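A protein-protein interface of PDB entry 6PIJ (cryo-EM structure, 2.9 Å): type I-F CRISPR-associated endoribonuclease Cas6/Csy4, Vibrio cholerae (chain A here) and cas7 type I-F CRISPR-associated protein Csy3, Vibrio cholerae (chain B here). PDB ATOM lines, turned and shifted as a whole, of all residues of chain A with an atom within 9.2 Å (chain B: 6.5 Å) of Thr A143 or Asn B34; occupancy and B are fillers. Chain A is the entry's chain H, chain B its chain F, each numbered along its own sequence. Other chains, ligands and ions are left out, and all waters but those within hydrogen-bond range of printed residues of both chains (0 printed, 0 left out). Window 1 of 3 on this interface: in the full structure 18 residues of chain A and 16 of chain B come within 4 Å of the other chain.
Printed residues of chain B that touch a printed residue of chain A: Thr B32, Tyr B33, Asn B34, Ser B35, Arg B36, Thr B37, Leu B38, His B76 and Arg B254.
Hydrophobic or aromatic side chains of chain B within 4 Å of the printed part of chain A: Leu B38 and His B76.
The side-chain carboxylate (OE1) of Glu A141 lies within salt-bridge range of the guanidinium group (NH2) of Arg B254, at 3.3 Å.
The backbone carbonyl oxygen (O) of Thr A143 sits at hydrogen-bond distance from the backbone NH (N) of Thr B37.
N of Ser B35 is in hydrogen-bond range of O of Glu A141 (3.1 Å).
ND1 of His A142 sits at hydrogen-bond distance from O of Ser B35, at 3.4 Å.
The backbone carbonyl oxygen (O) of Thr B37 lies within hydrogen-bond range of the backbone NH (N) of Ile A145.
Leu A109 touches none of the printed residues of chain B.
Of the printed residues of chain B, Glu A141 touches Asn B34 (3.8 Å), Ser B35 (3.1 Å) and Arg B254 (2.6 Å).
Thr A143 touches four residues of chain B.
Of the printed residues of chain B, Ala A144 touches Thr B37.
Of the printed residues of chain A, Asn B34 touches Gln A139 (3.6 Å), Glu A141 (3.8 Å), His A142 (3.9 Å) and Thr A143 (3.96 Å).
Ser B35 touches just these residues of chain A: Glu A141, His A142 and Thr A143.
Printed residues of chain A within 4 Å of Arg B36: Thr A143.
Asp B73 touches none of the printed residues of chain A.
The nearest residue of chain B that does not touch Thr A143 is Leu B38 (5.3 Å).
The nearest printed residue of chain B that does not touch Ala A144 is Leu B38 (5.6 Å).
N of Phe B74 is in hydrogen-bond range of O of Asn B34, at 2.8 Å.
N of Arg B36 lies within hydrogen-bond range of O of Val B72 (2.8 Å).
NH1 of Arg B254 lies within hydrogen-bond range of OH of Tyr B33.
OG1 of Thr B32 lies within hydrogen-bond range of O of Arg B254.
The side-chain carboxylate (OD1) of Asp B73 sits at hydrogen-bond distance from the side-chain hydroxyl (OG) of Ser B35, at 3.2 Å.
Ala A111 touches His B76.
Gln A139 touches Thr B32 (NE2 to O, 3.7 Å).
Gln A139 touches Tyr B33.
Asn B34 touches Gln A139.
Asn B34 touches Glu A141 (OD1 to O, 3.8 Å).
Asn B34 touches His A142.
His A142 touches Thr B37 (CE1 to OG1, 3.6 Å).
CA of Ala A144 touches O of Thr B37 (3.4 Å).
CA of Leu B38 touches O of Ile A145, 3.2 Å away.
Tyr A148 touches Leu B38.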
ATOM      1  N   ILE A 106     -19.655 -24.952 -32.179  1.00  0.00           N
ATOM      2  CA  ILE A 106     -20.793 -24.261 -31.496  1.00  0.00           C
ATOM      3  C   ILE A 106     -21.633 -25.303 -30.748  1.00  0.00           C
ATOM      4  O   ILE A 106     -22.143 -24.971 -29.659  1.00  0.00           O
ATOM      5  CB  ILE A 106     -21.625 -23.450 -32.518  1.00  0.00           C
ATOM      6  CG1 ILE A 106     -20.750 -22.546 -33.398  1.00  0.00           C
ATOM      7  CG2 ILE A 106     -22.734 -22.662 -31.834  1.00  0.00           C
ATOM      8  CD1 ILE A 106     -19.650 -21.796 -32.662  1.00  0.00           C
ATOM      9  N   LYS A 108     -20.550 -27.967 -29.252  1.00  0.00           N
ATOM     10  CA  LYS A 108     -19.770 -28.397 -28.056  1.00  0.00           C
ATOM     11  C   LYS A 108     -19.485 -27.200 -27.130  1.00  0.00           C
ATOM     12  O   LYS A 108     -18.590 -27.337 -26.269  1.00  0.00           O
ATOM     13  CB  LYS A 108     -18.490 -29.130 -28.486  1.00  0.00           C
ATOM     14  CG  LYS A 108     -17.498 -28.340 -29.333  1.00  0.00           C
ATOM     15  CD  LYS A 108     -16.236 -29.116 -29.657  1.00  0.00           C
ATOM     16  CE  LYS A 108     -15.080 -28.229 -30.068  1.00  0.00           C
ATOM     17  NZ  LYS A 108     -13.957 -29.016 -30.628  1.00  0.00           N
ATOM     18  N   LEU A 109     -20.213 -26.081 -27.281  1.00  0.00           N
ATOM     19  CA  LEU A 109     -20.237 -24.948 -26.310  1.00  0.00           C
ATOM     20  C   LEU A 109     -21.494 -25.022 -25.434  1.00  0.00           C
ATOM     21  O   LEU A 109     -21.430 -24.515 -24.296  1.00  0.00           O
ATOM     22  CB  LEU A 109     -20.175 -23.606 -27.049  1.00  0.00           C
ATOM     23  CG  LEU A 109     -18.807 -23.190 -27.591  1.00  0.00           C
ATOM     24  CD1 LEU A 109     -18.872 -21.783 -28.166  1.00  0.00           C
ATOM     25  CD2 LEU A 109     -17.728 -23.276 -26.519  1.00  0.00           C
ATOM     26  N   THR A 110     -22.590 -25.601 -25.944  1.00  0.00           N
ATOM     27  CA  THR A 110     -23.831 -25.896 -25.171  1.00  0.00           C
ATOM     28  C   THR A 110     -23.459 -26.743 -23.946  1.00  0.00           C
ATOM     29  O   THR A 110     -22.506 -27.558 -24.045  1.00  0.00           O
ATOM     30  CB  THR A 110     -24.896 -26.568 -26.050  1.00  0.00           C
ATOM     31  OG1 THR A 110     -25.031 -25.811 -27.254  1.00  0.00           O
ATOM     32  CG2 THR A 110     -26.245 -26.675 -25.372  1.00  0.00           C
ATOM     33  N   ALA A 111     -24.168 -26.536 -22.831  1.00  0.00           N
ATOM     34  CA  ALA A 111     -23.913 -27.168 -21.511  1.00  0.00           C
ATOM     35  C   ALA A 111     -23.894 -28.696 -21.646  1.00  0.00           C
ATOM     36  O   ALA A 111     -23.017 -29.332 -21.023  1.00  0.00           O
ATOM     37  CB  ALA A 111     -24.953 -26.719 -20.514  1.00  0.00           C
ATOM     38  N   ALA A 112     -24.828 -29.251 -22.430  1.00  0.00           N
ATOM     39  CA  ALA A 112     -24.881 -30.676 -22.836  1.00  0.00           C
ATOM     40  C   ALA A 112     -23.575 -31.057 -23.545  1.00  0.00           C
ATOM     41  O   ALA A 112     -22.980 -32.094 -23.179  1.00  0.00           O
ATOM     42  CB  ALA A 112     -26.078 -30.914 -23.725  1.00  0.00           C
ATOM     43  N   LEU A 114     -20.569 -29.497 -23.413  1.00  0.00           N
ATOM     44  CA  LEU A 114     -19.458 -29.454 -22.417  1.00  0.00           C
ATOM     45  C   LEU A 114     -19.448 -30.764 -21.613  1.00  0.00           C
ATOM     46  O   LEU A 114     -18.374 -31.408 -21.542  1.00  0.00           O
ATOM     47  CB  LEU A 114     -19.613 -28.233 -21.501  1.00  0.00           C
ATOM     48  CG  LEU A 114     -18.650 -28.154 -20.312  1.00  0.00           C
ATOM     49  CD1 LEU A 114     -17.197 -28.233 -20.763  1.00  0.00           C
ATOM     50  CD2 LEU A 114     -18.882 -26.885 -19.506  1.00  0.00           C
ATOM     51  N   ALA A 138     -14.754 -25.790 -15.505  1.00  0.00           N
ATOM     52  CA  ALA A 138     -15.831 -24.782 -15.393  1.00  0.00           C
ATOM     53  C   ALA A 138     -15.881 -23.945 -16.674  1.00  0.00           C
ATOM     54  O   ALA A 138     -14.818 -23.434 -17.085  1.00  0.00           O
ATOM     55  CB  ALA A 138     -15.593 -23.916 -14.181  1.00  0.00           C
ATOM     56  N   GLN A 139     -17.066 -23.847 -17.288  1.00  0.00           N
ATOM     57  CA  GLN A 139     -17.434 -22.781 -18.260  1.00  0.00           C
ATOM     58  C   GLN A 139     -16.955 -21.438 -17.694  1.00  0.00           C
ATOM     59  O   GLN A 139     -17.248 -21.168 -16.511  1.00  0.00           O
ATOM     60  CB  GLN A 139     -18.943 -22.798 -18.526  1.00  0.00           C
ATOM     61  CG  GLN A 139     -19.805 -22.604 -17.279  1.00  0.00           C
ATOM     62  CD  GLN A 139     -21.162 -23.265 -17.353  1.00  0.00           C
ATOM     63  OE1 GLN A 139     -21.582 -23.776 -18.390  1.00  0.00           O
ATOM     64  NE2 GLN A 139     -21.873 -23.250 -16.237  1.00  0.00           N
ATOM     65  N   LYS A 140     -16.237 -20.651 -18.506  1.00  0.00           N
ATOM     66  CA  LYS A 140     -15.409 -19.485 -18.077  1.00  0.00           C
ATOM     67  C   LYS A 140     -16.284 -18.529 -17.250  1.00  0.00           C
ATOM     68  O   LYS A 140     -16.339 -18.701 -16.016  1.00  0.00           O
ATOM     69  CB  LYS A 140     -14.778 -18.801 -19.298  1.00  0.00           C
ATOM     70  CG  LYS A 140     -13.837 -19.652 -20.143  1.00  0.00           C
ATOM     71  CD  LYS A 140     -13.372 -18.966 -21.419  1.00  0.00           C
ATOM     72  CE  LYS A 140     -14.473 -18.716 -22.434  1.00  0.00           C
ATOM     73  NZ  LYS A 140     -15.118 -19.972 -22.887  1.00  0.00           N
ATOM     74  N   GLU A 141     -16.885 -17.527 -17.896  1.00  0.00           N
ATOM     75  CA  GLU A 141     -18.124 -16.838 -17.438  1.00  0.00           C
ATOM     76  C   GLU A 141     -18.880 -16.218 -18.628  1.00  0.00           C
ATOM     77  O   GLU A 141     -20.071 -15.907 -18.449  1.00  0.00           O
ATOM     78  CB  GLU A 141     -17.775 -15.786 -16.380  1.00  0.00           C
ATOM     79  CG  GLU A 141     -16.962 -14.609 -16.906  1.00  0.00           C
ATOM     80  CD  GLU A 141     -17.718 -13.311 -17.152  1.00  0.00           C
ATOM     81  OE1 GLU A 141     -18.967 -13.327 -17.136  1.00  0.00           O
ATOM     82  OE2 GLU A 141     -17.051 -12.280 -17.366  1.00  0.00           O
ATOM     83  N   HIS A 142     -18.234 -16.066 -19.793  1.00  0.00           N
ATOM     84  CA  HIS A 142     -18.694 -15.220 -20.926  1.00  0.00           C
ATOM     85  C   HIS A 142     -18.134 -15.764 -22.246  1.00  0.00           C
ATOM     86  O   HIS A 142     -16.919 -16.044 -22.294  1.00  0.00           O
ATOM     87  CB  HIS A 142     -18.266 -13.768 -20.681  1.00  0.00           C
ATOM     88  CG  HIS A 142     -18.973 -12.767 -21.530  1.00  0.00           C
ATOM     89  ND1 HIS A 142     -20.183 -12.212 -21.159  1.00  0.00           N
ATOM     90  CD2 HIS A 142     -18.643 -12.207 -22.714  1.00  0.00           C
ATOM     91  CE1 HIS A 142     -20.573 -11.359 -22.083  1.00  0.00           C
ATOM     92  NE2 HIS A 142     -19.645 -11.337 -23.049  1.00  0.00           N
ATOM     93  N   THR A 143     -18.990 -15.908 -23.265  1.00  0.00           N
ATOM     94  CA  THR A 143     -18.630 -16.358 -24.638  1.00  0.00           C
ATOM     95  C   THR A 143     -19.303 -15.440 -25.667  1.00  0.00           C
ATOM     96  O   THR A 143     -20.549 -15.390 -25.679  1.00  0.00           O
ATOM     97  CB  THR A 143     -19.020 -17.826 -24.867  1.00  0.00           C
ATOM     98  OG1 THR A 143     -20.444 -17.933 -24.865  1.00  0.00           O
ATOM     99  CG2 THR A 143     -18.444 -18.764 -23.829  1.00  0.00           C
ATOM    100  N   ALA A 144     -18.506 -14.743 -26.486  1.00  0.00           N
ATOM    101  CA  ALA A 144     -18.964 -13.906 -27.622  1.00  0.00           C
ATOM    102  C   ALA A 144     -18.897 -14.740 -28.910  1.00  0.00           C
ATOM    103  O   ALA A 144     -17.773 -15.024 -29.371  1.00  0.00           O
ATOM    104  CB  ALA A 144     -18.131 -12.651 -27.718  1.00  0.00           C
ATOM    105  N   ILE A 145     -20.062 -15.113 -29.457  1.00  0.00           N
ATOM    106  CA  ILE A 145     -20.222 -16.076 -30.591  1.00  0.00           C
ATOM    107  C   ILE A 145     -20.831 -15.332 -31.787  1.00  0.00           C
ATOM    108  O   ILE A 145     -21.577 -14.368 -31.558  1.00  0.00           O
ATOM    109  CB  ILE A 145     -21.091 -17.279 -30.161  1.00  0.00           C
ATOM    110  CG1 ILE A 145     -20.654 -17.864 -28.813  1.00  0.00           C
ATOM    111  CG2 ILE A 145     -21.128 -18.345 -31.246  1.00  0.00           C
ATOM    112  CD1 ILE A 145     -19.232 -18.386 -28.787  1.00  0.00           C
ATOM    113  N   ALA A 146     -20.514 -15.763 -33.013  1.00  0.00           N
ATOM    114  CA  ALA A 146     -21.081 -15.243 -34.282  1.00  0.00           C
ATOM    115  C   ALA A 146     -20.692 -16.170 -35.429  1.00  0.00           C
ATOM    116  O   ALA A 146     -19.518 -16.520 -35.522  1.00  0.00           O
ATOM    117  CB  ALA A 146     -20.572 -13.850 -34.544  1.00  0.00           C
ATOM    118  N   TYR A 148     -23.641 -18.070 -37.607  1.00  0.00           N
ATOM    119  CA  TYR A 148     -23.811 -19.552 -37.593  1.00  0.00           C
ATOM    120  C   TYR A 148     -25.236 -20.023 -37.933  1.00  0.00           C
ATOM    121  O   TYR A 148     -25.362 -21.254 -38.083  1.00  0.00           O
ATOM    122  CB  TYR A 148     -23.261 -20.166 -36.297  1.00  0.00           C
ATOM    123  CG  TYR A 148     -24.108 -20.097 -35.047  1.00  0.00           C
ATOM    124  CD1 TYR A 148     -25.209 -20.924 -34.867  1.00  0.00           C
ATOM    125  CD2 TYR A 148     -23.762 -19.257 -33.999  1.00  0.00           C
ATOM    126  CE1 TYR A 148     -25.969 -20.882 -33.709  1.00  0.00           C
ATOM    127  CE2 TYR A 148     -24.512 -19.202 -32.833  1.00  0.00           C
ATOM    128  CZ  TYR A 148     -25.620 -20.019 -32.686  1.00  0.00           C
ATOM    129  OH  TYR A 148     -26.362 -19.972 -31.542  1.00  0.00           O
ATOM    130  N   THR B  32     -21.750 -21.638 -10.259  1.00  0.00           N
ATOM    131  CA  THR B  32     -21.513 -20.567 -11.267  1.00  0.00           C
ATOM    132  C   THR B  32     -22.195 -20.972 -12.579  1.00  0.00           C
ATOM    133  O   THR B  32     -22.452 -22.180 -12.765  1.00  0.00           O
ATOM    134  CB  THR B  32     -20.014 -20.265 -11.424  1.00  0.00           C
ATOM    135  OG1 THR B  32     -19.887 -19.135 -12.290  1.00  0.00           O
ATOM    136  CG2 THR B  32     -19.206 -21.421 -11.973  1.00  0.00           C
ATOM    137  N   TYR B  33     -22.466 -19.991 -13.446  1.00  0.00           N
ATOM    138  CA  TYR B  33     -23.270 -20.135 -14.690  1.00  0.00           C
ATOM    139  C   TYR B  33     -22.536 -19.491 -15.871  1.00  0.00           C
ATOM    140  O   TYR B  33     -21.604 -18.693 -15.642  1.00  0.00           O
ATOM    141  CB  TYR B  33     -24.657 -19.512 -14.499  1.00  0.00           C
ATOM    142  CG  TYR B  33     -24.662 -18.024 -14.247  1.00  0.00           C
ATOM    143  CD1 TYR B  33     -24.423 -17.513 -12.981  1.00  0.00           C
ATOM    144  CD2 TYR B  33     -24.920 -17.123 -15.268  1.00  0.00           C
ATOM    145  CE1 TYR B  33     -24.431 -16.149 -12.735  1.00  0.00           C
ATOM    146  CE2 TYR B  33     -24.933 -15.754 -15.040  1.00  0.00           C
ATOM    147  CZ  TYR B  33     -24.687 -15.265 -13.769  1.00  0.00           C
ATOM    148  OH  TYR B  33     -24.700 -13.920 -13.539  1.00  0.00           O
ATOM    149  N   ASN B  34     -22.965 -19.827 -17.094  1.00  0.00           N
ATOM    150  CA  ASN B  34     -22.403 -19.295 -18.367  1.00  0.00           C
ATOM    151  C   ASN B  34     -23.312 -18.172 -18.879  1.00  0.00           C
ATOM    152  O   ASN B  34     -24.538 -18.297 -18.711  1.00  0.00           O
ATOM    153  CB  ASN B  34     -22.243 -20.401 -19.415  1.00  0.00           C
ATOM    154  CG  ASN B  34     -21.410 -19.995 -20.614  1.00  0.00           C
ATOM    155  OD1 ASN B  34     -20.706 -18.988 -20.590  1.00  0.00           O
ATOM    156  ND2 ASN B  34     -21.475 -20.787 -21.672  1.00  0.00           N
ATOM    157  N   SER B  35     -22.725 -17.126 -19.475  1.00  0.00           N
ATOM    158  CA  SER B  35     -23.428 -15.945 -20.044  1.00  0.00           C
ATOM    159  C   SER B  35     -22.994 -15.727 -21.497  1.00  0.00           C
ATOM    160  O   SER B  35     -22.023 -14.977 -21.722  1.00  0.00           O
ATOM    161  CB  SER B  35     -23.183 -14.716 -19.207  1.00  0.00           C
ATOM    162  OG  SER B  35     -23.731 -13.563 -19.820  1.00  0.00           O
ATOM    163  N   ARG B  36     -23.706 -16.344 -22.445  1.00  0.00           N
ATOM    164  CA  ARG B  36     -23.404 -16.274 -23.899  1.00  0.00           C
ATOM    165  C   ARG B  36     -24.034 -15.011 -24.502  1.00  0.00           C
ATOM    166  O   ARG B  36     -25.148 -14.620 -24.060  1.00  0.00           O
ATOM    167  CB  ARG B  36     -23.923 -17.513 -24.634  1.00  0.00           C
ATOM    168  CG  ARG B  36     -23.489 -18.844 -24.033  1.00  0.00           C
ATOM    169  CD  ARG B  36     -23.572 -19.957 -25.063  1.00  0.00           C
ATOM    170  NE  ARG B  36     -24.885 -19.981 -25.706  1.00  0.00           N
ATOM    171  CZ  ARG B  36     -25.151 -20.377 -26.953  1.00  0.00           C
ATOM    172  NH1 ARG B  36     -26.400 -20.335 -27.393  1.00  0.00           N
ATOM    173  NH2 ARG B  36     -24.194 -20.803 -27.764  1.00  0.00           N
ATOM    174  N   THR B  37     -23.341 -14.415 -25.480  1.00  0.00           N
ATOM    175  CA  THR B  37     -23.798 -13.262 -26.304  1.00  0.00           C
ATOM    176  C   THR B  37     -23.489 -13.556 -27.777  1.00  0.00           C
ATOM    177  O   THR B  37     -22.328 -13.898 -28.072  1.00  0.00           O
ATOM    178  CB  THR B  37     -23.131 -11.956 -25.854  1.00  0.00           C
ATOM    179  OG1 THR B  37     -23.295 -11.829 -24.441  1.00  0.00           O
ATOM    180  CG2 THR B  37     -23.700 -10.734 -26.542  1.00  0.00           C
ATOM    181  N   LEU B  38     -24.488 -13.430 -28.658  1.00  0.00           N
ATOM    182  CA  LEU B  38     -24.339 -13.629 -30.126  1.00  0.00           C
ATOM    183  C   LEU B  38     -23.901 -12.303 -30.764  1.00  0.00           C
ATOM    184  O   LEU B  38     -24.774 -11.443 -31.010  1.00  0.00           O
ATOM    185  CB  LEU B  38     -25.658 -14.150 -30.710  1.00  0.00           C
ATOM    186  CG  LEU B  38     -26.150 -15.485 -30.149  1.00  0.00           C
ATOM    187  CD1 LEU B  38     -27.454 -15.903 -30.814  1.00  0.00           C
ATOM    188  CD2 LEU B  38     -25.098 -16.575 -30.308  1.00  0.00           C
ATOM    189  N   VAL B  72     -27.694 -13.965 -23.023  1.00  0.00           N
ATOM    190  CA  VAL B  72     -28.491 -15.129 -22.523  1.00  0.00           C
ATOM    191  C   VAL B  72     -27.622 -15.939 -21.553  1.00  0.00           C
ATOM    192  O   VAL B  72     -26.440 -16.169 -21.873  1.00  0.00           O
ATOM    193  CB  VAL B  72     -29.031 -16.008 -23.669  1.00  0.00           C
ATOM    194  CG1 VAL B  72     -29.980 -17.083 -23.155  1.00  0.00           C
ATOM    195  CG2 VAL B  72     -29.710 -15.181 -24.754  1.00  0.00           C
ATOM    196  N   ASP B  73     -28.204 -16.357 -20.421  1.00  0.00           N
ATOM    197  CA  ASP B  73     -27.512 -17.076 -19.317  1.00  0.00           C
ATOM    198  C   ASP B  73     -27.986 -18.534 -19.272  1.00  0.00           C
ATOM    199  O   ASP B  73     -29.178 -18.778 -19.542  1.00  0.00           O
ATOM    200  CB  ASP B  73     -27.748 -16.385 -17.971  1.00  0.00           C
ATOM    201  CG  ASP B  73     -27.220 -14.961 -17.884  1.00  0.00           C
ATOM    202  OD1 ASP B  73     -26.630 -14.482 -18.875  1.00  0.00           O
ATOM    203  OD2 ASP B  73     -27.400 -14.340 -16.819  1.00  0.00           O
ATOM    204  N   PHE B  74     -27.072 -19.456 -18.948  1.00  0.00           N
ATOM    205  CA  PHE B  74     -27.316 -20.918 -18.810  1.00  0.00           C
ATOM    206  C   PHE B  74     -26.630 -21.412 -17.532  1.00  0.00           C
ATOM    207  O   PHE B  74     -25.399 -21.202 -17.391  1.00  0.00           O
ATOM    208  CB  PHE B  74     -26.806 -21.675 -20.041  1.00  0.00           C
ATOM    209  CG  PHE B  74     -27.329 -21.160 -21.358  1.00  0.00           C
ATOM    210  CD1 PHE B  74     -26.766 -20.040 -21.953  1.00  0.00           C
ATOM    211  CD2 PHE B  74     -28.387 -21.786 -22.002  1.00  0.00           C
ATOM    212  CE1 PHE B  74     -27.253 -19.553 -23.156  1.00  0.00           C
ATOM    213  CE2 PHE B  74     -28.866 -21.305 -23.212  1.00  0.00           C
ATOM    214  CZ  PHE B  74     -28.299 -20.189 -23.787  1.00  0.00           C
ATOM    215  N   CYS B  75     -27.407 -22.032 -16.636  1.00  0.00           N
ATOM    216  CA  CYS B  75     -26.967 -22.564 -15.318  1.00  0.00           C
ATOM    217  C   CYS B  75     -27.386 -24.034 -15.191  1.00  0.00           C
ATOM    218  O   CYS B  75     -28.585 -24.296 -14.946  1.00  0.00           O
ATOM    219  CB  CYS B  75     -27.546 -21.740 -14.174  1.00  0.00           C
ATOM    220  SG  CYS B  75     -26.871 -22.189 -12.554  1.00  0.00           S
ATOM    221  N   HIS B  76     -26.429 -24.949 -15.371  1.00  0.00           N
ATOM    222  CA  HIS B  76     -26.591 -26.418 -15.202  1.00  0.00           C
ATOM    223  C   HIS B  76     -25.727 -26.899 -14.033  1.00  0.00           C
ATOM    224  O   HIS B  76     -24.857 -26.126 -13.579  1.00  0.00           O
ATOM    225  CB  HIS B  76     -26.240 -27.146 -16.506  1.00  0.00           C
ATOM    226  CG  HIS B  76     -27.179 -26.854 -17.627  1.00  0.00           C
ATOM    227  ND1 HIS B  76     -27.036 -25.747 -18.439  1.00  0.00           N
ATOM    228  CD2 HIS B  76     -28.271 -27.514 -18.071  1.00  0.00           C
ATOM    229  CE1 HIS B  76     -27.997 -25.740 -19.341  1.00  0.00           C
ATOM    230  NE2 HIS B  76     -28.770 -26.813 -19.135  1.00  0.00           N
ATOM    231  N   PHE B 245     -29.637 -13.372 -15.310  1.00  0.00           N
ATOM    232  CA  PHE B 245     -29.893 -13.902 -13.944  1.00  0.00           C
ATOM    233  C   PHE B 245     -29.517 -12.861 -12.886  1.00  0.00           C
ATOM    234  O   PHE B 245     -28.575 -12.074 -13.109  1.00  0.00           O
ATOM    235  CB  PHE B 245     -29.113 -15.196 -13.684  1.00  0.00           C
ATOM    236  CG  PHE B 245     -29.506 -16.398 -14.509  1.00  0.00           C
ATOM    237  CD1 PHE B 245     -30.812 -16.595 -14.945  1.00  0.00           C
ATOM    238  CD2 PHE B 245     -28.564 -17.373 -14.809  1.00  0.00           C
ATOM    239  CE1 PHE B 245     -31.153 -17.718 -15.685  1.00  0.00           C
ATOM    240  CE2 PHE B 245     -28.908 -18.494 -15.549  1.00  0.00           C
ATOM    241  CZ  PHE B 245     -30.201 -18.665 -15.987  1.00  0.00           C
ATOM    242  N   ARG B 254     -19.081 -15.047  -9.089  1.00  0.00           N
ATOM    243  CA  ARG B 254     -20.529 -14.719  -9.170  1.00  0.00           C
ATOM    244  C   ARG B 254     -21.335 -16.023  -9.144  1.00  0.00           C
ATOM    245  O   ARG B 254     -20.871 -17.021  -9.734  1.00  0.00           O
ATOM    246  CB  ARG B 254     -20.858 -13.858 -10.398  1.00  0.00           C
ATOM    247  CG  ARG B 254     -20.503 -14.486 -11.737  1.00  0.00           C
ATOM    248  CD  ARG B 254     -21.241 -13.864 -12.905  1.00  0.00           C
ATOM    249  NE  ARG B 254     -21.078 -14.696 -14.089  1.00  0.00           N
ATOM    250  CZ  ARG B 254     -21.636 -14.474 -15.276  1.00  0.00           C
ATOM    251  NH1 ARG B 254     -22.418 -13.425 -15.480  1.00  0.00           N
ATOM    252  NH2 ARG B 254     -21.399 -15.322 -16.262  1.00  0.00           N
